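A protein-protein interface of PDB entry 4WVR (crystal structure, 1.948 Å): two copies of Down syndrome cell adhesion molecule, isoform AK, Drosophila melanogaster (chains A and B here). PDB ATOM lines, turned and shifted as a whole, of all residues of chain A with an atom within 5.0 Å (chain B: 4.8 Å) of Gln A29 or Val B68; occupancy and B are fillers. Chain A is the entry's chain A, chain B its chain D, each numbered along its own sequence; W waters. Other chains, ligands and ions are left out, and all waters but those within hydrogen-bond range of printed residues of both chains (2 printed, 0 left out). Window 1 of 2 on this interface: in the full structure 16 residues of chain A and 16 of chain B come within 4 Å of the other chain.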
ATOM      1  N   ALA A  11      12.907  -9.537  34.304  1.00  0.00           N
ATOM      2  CA  ALA A  11      13.106  -9.016  32.958  1.00  0.00           C
ATOM      3  C   ALA A  11      11.752  -8.754  32.309  1.00  0.00           C
ATOM      4  O   ALA A  11      10.852  -9.592  32.378  1.00  0.00           O
ATOM      5  CB  ALA A  11      13.925  -9.985  32.116  1.00  0.00           C
ATOM      6  N   PHE A  13       8.798  -8.421  29.529  1.00  0.00           N
ATOM      7  CA  PHE A  13       8.429  -9.218  28.367  1.00  0.00           C
ATOM      8  C   PHE A  13       7.346  -8.502  27.572  1.00  0.00           C
ATOM      9  O   PHE A  13       6.773  -7.523  28.042  1.00  0.00           O
ATOM     10  CB  PHE A  13       7.962 -10.622  28.782  1.00  0.00           C
ATOM     11  CG  PHE A  13       6.920 -10.636  29.878  1.00  0.00           C
ATOM     12  CD1 PHE A  13       5.624 -10.204  29.638  1.00  0.00           C
ATOM     13  CD2 PHE A  13       7.233 -11.121  31.139  1.00  0.00           C
ATOM     14  CE1 PHE A  13       4.664 -10.231  30.639  1.00  0.00           C
ATOM     15  CE2 PHE A  13       6.277 -11.160  32.145  1.00  0.00           C
ATOM     16  CZ  PHE A  13       4.992 -10.710  31.894  1.00  0.00           C
ATOM     17  N   GLY A  27       2.857 -16.076  23.494  1.00  0.00           N
ATOM     18  CA  GLY A  27       3.412 -16.435  24.784  1.00  0.00           C
ATOM     19  C   GLY A  27       4.518 -15.518  25.256  1.00  0.00           C
ATOM     20  O   GLY A  27       5.058 -14.727  24.479  1.00  0.00           O
ATOM     21  N   VAL A  28       4.843 -15.627  26.542  1.00  0.00           N
ATOM     22  CA  VAL A  28       5.942 -14.884  27.149  1.00  0.00           C
ATOM     23  C   VAL A  28       6.639 -15.731  28.209  1.00  0.00           C
ATOM     24  O   VAL A  28       6.043 -16.673  28.748  1.00  0.00           O
ATOM     25  CB  VAL A  28       5.458 -13.576  27.808  1.00  0.00           C
ATOM     26  CG1 VAL A  28       5.079 -12.538  26.758  1.00  0.00           C
ATOM     27  CG2 VAL A  28       4.292 -13.854  28.754  1.00  0.00           C
ATOM     28  N   GLN A  29       7.899 -15.402  28.491  1.00  0.00           N
ATOM     29  CA  GLN A  29       8.632 -16.010  29.598  1.00  0.00           C
ATOM     30  C   GLN A  29       8.832 -14.975  30.681  1.00  0.00           C
ATOM     31  O   GLN A  29       9.357 -13.891  30.416  1.00  0.00           O
ATOM     32  CB  GLN A  29      10.008 -16.524  29.180  1.00  0.00           C
ATOM     33  CG  GLN A  29      10.025 -17.759  28.305  1.00  0.00           C
ATOM     34  CD  GLN A  29      11.392 -18.429  28.270  1.00  0.00           C
ATOM     35  OE1 GLN A  29      12.168 -18.374  29.228  1.00  0.00           O
ATOM     36  NE2 GLN A  29      11.728 -18.984  27.120  1.00  0.00           N
ATOM     37  N   CYS A  30       8.437 -15.313  31.903  1.00  0.00           N
ATOM     38  CA  CYS A  30       8.734 -14.472  33.056  1.00  0.00           C
ATOM     39  C   CYS A  30      10.041 -14.942  33.671  1.00  0.00           C
ATOM     40  O   CYS A  30      10.088 -15.972  34.347  1.00  0.00           O
ATOM     41  CB  CYS A  30       7.600 -14.526  34.080  1.00  0.00           C
ATOM     42  SG  CYS A  30       7.856 -13.459  35.514  1.00  0.00           S
ATOM     43  N   MET A  31      11.108 -14.196  33.421  1.00  0.00           N
ATOM     44  CA  MET A  31      12.431 -14.614  33.860  1.00  0.00           C
ATOM     45  C   MET A  31      12.952 -13.709  34.964  1.00  0.00           C
ATOM     46  O   MET A  31      13.306 -12.554  34.730  1.00  0.00           O
ATOM     47  CB  MET A  31      13.404 -14.643  32.678  1.00  0.00           C
ATOM     48  CG  MET A  31      13.138 -15.790  31.699  1.00  0.00           C
ATOM     49  SD  MET A  31      14.076 -15.651  30.161  1.00  0.00           S
ATOM     50  CE  MET A  31      13.257 -14.251  29.397  1.00  0.00           C
ATOM     51  N   TRP A  43       0.573 -15.663  37.870  1.00  0.00           N
ATOM     52  CA  TRP A  43       0.090 -14.812  36.795  1.00  0.00           C
ATOM     53  C   TRP A  43      -1.318 -14.288  37.052  1.00  0.00           C
ATOM     54  O   TRP A  43      -2.133 -14.948  37.699  1.00  0.00           O
ATOM     55  CB  TRP A  43       0.110 -15.576  35.469  1.00  0.00           C
ATOM     56  CG  TRP A  43       1.477 -15.962  34.988  1.00  0.00           C
ATOM     57  CD1 TRP A  43       2.205 -17.054  35.369  1.00  0.00           C
ATOM     58  CD2 TRP A  43       2.271 -15.271  34.017  1.00  0.00           C
ATOM     59  NE1 TRP A  43       3.404 -17.080  34.701  1.00  0.00           N
ATOM     60  CE2 TRP A  43       3.469 -15.997  33.863  1.00  0.00           C
ATOM     61  CE3 TRP A  43       2.088 -14.104  33.267  1.00  0.00           C
ATOM     62  CZ2 TRP A  43       4.480 -15.595  32.990  1.00  0.00           C
ATOM     63  CZ3 TRP A  43       3.094 -13.707  32.394  1.00  0.00           C
ATOM     64  CH2 TRP A  43       4.274 -14.450  32.266  1.00  0.00           C
ATOM     65  N   LEU A  62       9.202 -23.339  34.709  1.00  0.00           N
ATOM     66  CA  LEU A  62      10.246 -24.005  33.943  1.00  0.00           C
ATOM     67  C   LEU A  62      11.495 -24.272  34.780  1.00  0.00           C
ATOM     68  O   LEU A  62      12.226 -25.235  34.543  1.00  0.00           O
ATOM     69  CB  LEU A  62      10.604 -23.157  32.722  1.00  0.00           C
ATOM     70  CG  LEU A  62      11.544 -23.777  31.689  1.00  0.00           C
ATOM     71  CD1 LEU A  62      10.911 -25.015  31.088  1.00  0.00           C
ATOM     72  CD2 LEU A  62      11.898 -22.769  30.607  1.00  0.00           C
ATOM     73  N   THR A  66      12.080 -19.114  36.477  1.00  0.00           N
ATOM     74  CA  THR A  66      11.426 -18.843  35.201  1.00  0.00           C
ATOM     75  C   THR A  66      10.060 -19.507  35.098  1.00  0.00           C
ATOM     76  O   THR A  66       9.911 -20.699  35.382  1.00  0.00           O
ATOM     77  CB  THR A  66      12.300 -19.305  34.021  1.00  0.00           C
ATOM     78  OG1 THR A  66      13.528 -18.564  34.021  1.00  0.00           O
ATOM     79  CG2 THR A  66      11.581 -19.078  32.696  1.00  0.00           C
ATOM     80  N   SER A  67       9.060 -18.724  34.704  1.00  0.00           N
ATOM     81  CA  SER A  67       7.738 -19.263  34.422  1.00  0.00           C
ATOM     82  C   SER A  67       7.329 -18.899  33.000  1.00  0.00           C
ATOM     83  O   SER A  67       7.520 -17.762  32.566  1.00  0.00           O
ATOM     84  CB  SER A  67       6.708 -18.739  35.422  1.00  0.00           C
ATOM     85  OG  SER A  67       5.403 -19.189  35.096  1.00  0.00           O
ATOM     86  N   VAL A  68       6.766 -19.868  32.285  1.00  0.00           N
ATOM     87  CA  VAL A  68       6.383 -19.676  30.887  1.00  0.00           C
ATOM     88  C   VAL A  68       4.871 -19.666  30.695  1.00  0.00           C
ATOM     89  O   VAL A  68       4.170 -20.567  31.155  1.00  0.00           O
ATOM     90  CB  VAL A  68       6.961 -20.780  29.992  1.00  0.00           C
ATOM     91  CG1 VAL A  68       6.741 -20.433  28.526  1.00  0.00           C
ATOM     92  CG2 VAL A  68       8.437 -20.979  30.287  1.00  0.00           C
ATOM     93  N   GLY B  27      16.191 -16.001  27.588  1.00  0.00           N
ATOM     94  CA  GLY B  27      15.441 -17.017  26.879  1.00  0.00           C
ATOM     95  C   GLY B  27      14.620 -16.525  25.703  1.00  0.00           C
ATOM     96  O   GLY B  27      14.325 -15.333  25.565  1.00  0.00           O
ATOM     97  N   VAL B  28      14.250 -17.469  24.847  1.00  0.00           N
ATOM     98  CA  VAL B  28      13.375 -17.206  23.717  1.00  0.00           C
ATOM     99  C   VAL B  28      12.406 -18.365  23.557  1.00  0.00           C
ATOM    100  O   VAL B  28      12.562 -19.410  24.192  1.00  0.00           O
ATOM    101  CB  VAL B  28      14.155 -17.022  22.398  1.00  0.00           C
ATOM    102  CG1 VAL B  28      14.930 -15.716  22.405  1.00  0.00           C
ATOM    103  CG2 VAL B  28      15.089 -18.215  22.158  1.00  0.00           C
ATOM    104  N   GLN B  29      11.414 -18.178  22.699  1.00  0.00           N
ATOM    105  CA  GLN B  29      10.420 -19.207  22.461  1.00  0.00           C
ATOM    106  C   GLN B  29      10.222 -19.412  20.963  1.00  0.00           C
ATOM    107  O   GLN B  29      10.159 -18.446  20.200  1.00  0.00           O
ATOM    108  CB  GLN B  29       9.104 -18.822  23.126  1.00  0.00           C
ATOM    109  CG  GLN B  29       8.726 -19.708  24.283  1.00  0.00           C
ATOM    110  CD  GLN B  29       7.466 -19.246  24.971  1.00  0.00           C
ATOM    111  OE1 GLN B  29       7.326 -18.075  25.337  1.00  0.00           O
ATOM    112  NE2 GLN B  29       6.520 -20.161  25.123  1.00  0.00           N
ATOM    113  N   THR B  58      18.453 -24.902  28.662  1.00  0.00           N
ATOM    114  CA  THR B  58      17.184 -25.602  28.822  1.00  0.00           C
ATOM    115  C   THR B  58      16.348 -25.492  27.551  1.00  0.00           C
ATOM    116  O   THR B  58      16.165 -24.402  27.012  1.00  0.00           O
ATOM    117  CB  THR B  58      16.373 -25.045  30.005  1.00  0.00           C
ATOM    118  OG1 THR B  58      17.121 -25.209  31.213  1.00  0.00           O
ATOM    119  CG2 THR B  58      15.034 -25.768  30.132  1.00  0.00           C
ATOM    120  N   ILE B  59      15.852 -26.628  27.074  1.00  0.00           N
ATOM    121  CA  ILE B  59      14.965 -26.670  25.921  1.00  0.00           C
ATOM    122  C   ILE B  59      13.802 -27.594  26.244  1.00  0.00           C
ATOM    123  O   ILE B  59      14.012 -28.759  26.556  1.00  0.00           O
ATOM    124  CB  ILE B  59      15.693 -27.163  24.656  1.00  0.00           C
ATOM    125  CG1 ILE B  59      16.783 -26.170  24.253  1.00  0.00           C
ATOM    126  CG2 ILE B  59      14.705 -27.356  23.507  1.00  0.00           C
ATOM    127  CD1 ILE B  59      17.661 -26.646  23.121  1.00  0.00           C
ATOM    128  N   LEU B  60      12.579 -27.072  26.184  1.00  0.00           N
ATOM    129  CA  LEU B  60      11.409 -27.844  26.588  1.00  0.00           C
ATOM    130  C   LEU B  60      10.256 -27.732  25.594  1.00  0.00           C
ATOM    131  O   LEU B  60       9.857 -26.629  25.214  1.00  0.00           O
ATOM    132  CB  LEU B  60      10.934 -27.398  27.973  1.00  0.00           C
ATOM    133  CG  LEU B  60       9.703 -28.130  28.515  1.00  0.00           C
ATOM    134  CD1 LEU B  60       9.950 -28.600  29.940  1.00  0.00           C
ATOM    135  CD2 LEU B  60       8.469 -27.240  28.449  1.00  0.00           C
ATOM    136  N   LEU B  62       6.777 -27.458  25.068  1.00  0.00           N
ATOM    137  CA  LEU B  62       5.635 -27.040  25.865  1.00  0.00           C
ATOM    138  C   LEU B  62       4.329 -27.546  25.246  1.00  0.00           C
ATOM    139  O   LEU B  62       3.377 -27.897  25.951  1.00  0.00           O
ATOM    140  CB  LEU B  62       5.646 -25.509  25.992  1.00  0.00           C
ATOM    141  CG  LEU B  62       4.795 -24.761  27.023  1.00  0.00           C
ATOM    142  CD1 LEU B  62       3.384 -24.553  26.501  1.00  0.00           C
ATOM    143  CD2 LEU B  62       4.788 -25.485  28.368  1.00  0.00           C
ATOM    144  N   THR B  66       5.033 -25.321  20.250  1.00  0.00           N
ATOM    145  CA  THR B  66       5.851 -24.377  21.010  1.00  0.00           C
ATOM    146  C   THR B  66       7.047 -25.041  21.694  1.00  0.00           C
ATOM    147  O   THR B  66       6.897 -25.987  22.475  1.00  0.00           O
ATOM    148  CB  THR B  66       5.019 -23.648  22.088  1.00  0.00           C
ATOM    149  OG1 THR B  66       3.972 -22.890  21.464  1.00  0.00           O
ATOM    150  CG2 THR B  66       5.903 -22.717  22.901  1.00  0.00           C
ATOM    151  N   SER B  67       8.236 -24.535  21.390  1.00  0.00           N
ATOM    152  CA  SER B  67       9.434 -24.940  22.107  1.00  0.00           C
ATOM    153  C   SER B  67       9.987 -23.753  22.878  1.00  0.00           C
ATOM    154  O   SER B  67      10.154 -22.662  22.327  1.00  0.00           O
ATOM    155  CB  SER B  67      10.493 -25.496  21.155  1.00  0.00           C
ATOM    156  OG  SER B  67      11.655 -25.867  21.880  1.00  0.00           O
ATOM    157  N   VAL B  68      10.261 -23.981  24.157  1.00  0.00           N
ATOM    158  CA  VAL B  68      10.767 -22.956  25.051  1.00  0.00           C
ATOM    159  C   VAL B  68      12.259 -23.133  25.300  1.00  0.00           C
ATOM    160  O   VAL B  68      12.699 -24.210  25.701  1.00  0.00           O
ATOM    161  CB  VAL B  68      10.019 -22.994  26.397  1.00  0.00           C
ATOM    162  CG1 VAL B  68      10.529 -21.912  27.317  1.00  0.00           C
ATOM    163  CG2 VAL B  68       8.518 -22.844  26.170  1.00  0.00           C
ATOM    164  N   LEU B  69      13.036 -22.081  25.064  1.00  0.00           N
ATOM    165  CA  LEU B  69      14.466 -22.123  25.347  1.00  0.00           C
ATOM    166  C   LEU B  69      14.808 -21.152  26.466  1.00  0.00           C
ATOM    167  O   LEU B  69      14.487 -19.963  26.397  1.00  0.00           O
ATOM    168  CB  LEU B  69      15.290 -21.803  24.091  1.00  0.00           C
ATOM    169  CG  LEU B  69      16.816 -21.979  24.192  1.00  0.00           C
ATOM    170  CD1 LEU B  69      17.427 -22.367  22.846  1.00  0.00           C
ATOM    171  CD2 LEU B  69      17.506 -20.724  24.730  1.00  0.00           C
ATOM    172  N   ASN B  70      15.471 -21.664  27.494  1.00  0.00           N
ATOM    173  CA  ASN B  70      15.891 -20.835  28.609  1.00  0.00           C
ATOM    174  C   ASN B  70      17.346 -21.085  28.973  1.00  0.00           C
ATOM    175  O   ASN B  70      17.781 -22.232  29.116  1.00  0.00           O
ATOM    176  CB  ASN B  70      15.001 -21.079  29.827  1.00  0.00           C
ATOM    177  CG  ASN B  70      15.408 -20.239  31.024  1.00  0.00           C
ATOM    178  OD1 ASN B  70      16.098 -20.715  31.931  1.00  0.00           O
ATOM    179  ND2 ASN B  70      14.994 -18.976  31.029  1.00  0.00           N
HETATM  180  O   HOH W   1      15.676 -19.947  34.557  1.00  0.00           O
HETATM  181  O   HOH W   2       8.376 -15.118  24.096  1.00  0.00           O
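Water W1 lies within hydrogen-bond range of OG1 of Thr A66 (2.6 Å) and OD1 of Asn B70 (2.8 Å). Water W2 bridges the backbone carbonyl oxygen of Gly A27 (3.4 Å) and the side-chain amide oxygen of Gln B29 (3.4 Å).
Gly A27 touches Gln B29, but with the chains exchanged Gln A29 does not touch Gly B27 (4.1 Å). Val A28 touches Gln B29, and with the chains exchanged Gln A29 touches Val B28. Gln A29 touches Val B68, and with the chains exchanged Val A68 touches Gln B29. Leu A62 touches Val B68, but with the chains exchanged Val A68 does not touch Leu B62 (5.0 Å).
Of the 12 printed residues of chain A, 7 touch a printed residue of chain B. Printed residues of chain A that touch a printed residue of chain B: Gly A27, Val A28, Gln A29, Met A31, Leu A62, Thr A66 and Val A68. Along chain A the printed residues that touch a printed residue of chain B span positions 27 to 68. Hydrophobic or aromatic side chains of chain B that line the printed part of chain A: Leu B60 and Val B68. Among the printed residues, no Asp or Glu carboxylate lies within 4 Å of a Lys or Arg side-chain nitrogen of the other chain.
Among the printed residues, pairs that only touch across the chains: Gln A29 with Val B68 (3.2 Å), Val A68 with Gln B29 (3.4 Å), Leu A62 with Asn B70 (3.6 Å), Leu A62 with Val B68 (3.7 Å), Val A28 with Gln B29 (3.7 Å), Val A68 with Val B68 (3.8 Å), Gly A27 with Gln B29 (3.8 Å) and Leu A62 with Leu B60 (3.9 Å).
The backbone carbonyl oxygen (O) of Met A31 lies within hydrogen-bond range of the backbone NH (N) of Ala A11 (3.1 Å). OE1 of Gln A29 lies close to SD of Met A31 (3.5 Å). O of Val B28 sits at hydrogen-bond distance from N of Leu B69, at 2.8 Å. The backbone carbonyl oxygen (O) of Asn B70 lies within hydrogen-bond range of the backbone NH (N) of Thr B58, at 2.8 Å. O of Leu B60 lies within hydrogen-bond range of N of Val B68 (2.9 Å).
The backbone carbonyl oxygen (O) of Val B28 is in hydrogen-bond range of the side-chain amide nitrogen (NE2) of Gln A29 (3.1 Å). The side-chain amide nitrogen (NE2) of Gln A29 lies within hydrogen-bond range of the backbone carbonyl oxygen (O) of Leu B69 (3.0 Å). The side-chain amide oxygen of Gln A29 is in hydrogen-bond range of the side-chain amide nitrogen of Asn B70 (3.4 Å). The backbone NH of Gly B27 sits at hydrogen-bond distance from the side-chain sulfur of Met A31 (3.3 Å). The side-chain amide nitrogen (ND2) of Asn B70 lies within hydrogen-bond range of the side-chain sulfur (SD) of Met A31, at 3.6 Å. ND2 of Asn B70 sits at hydrogen-bond distance from OG1 of Thr A66 (3.4 Å).
Of chain B, only Val B28, Val B68, Leu B69 and Asn B70 come within 4 Å of Gln A29. Of the printed residues of chain B, Met A31 touches Gly B27 and Asn B70. Of the printed residues of chain B, Thr A66 touches Asn B70. Printed residues of chain A within 4 Å of Gly B27: Met A31 (3.3 Å). Val B68 touches three residues of chain A. Printed residues of chain A within 4 Å of Asn B70: Gln A29, Met A31, Leu A62 and Thr A66. The nearest printed residue of chain A that does not touch Val B68 is Thr A66 (6.2 Å).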
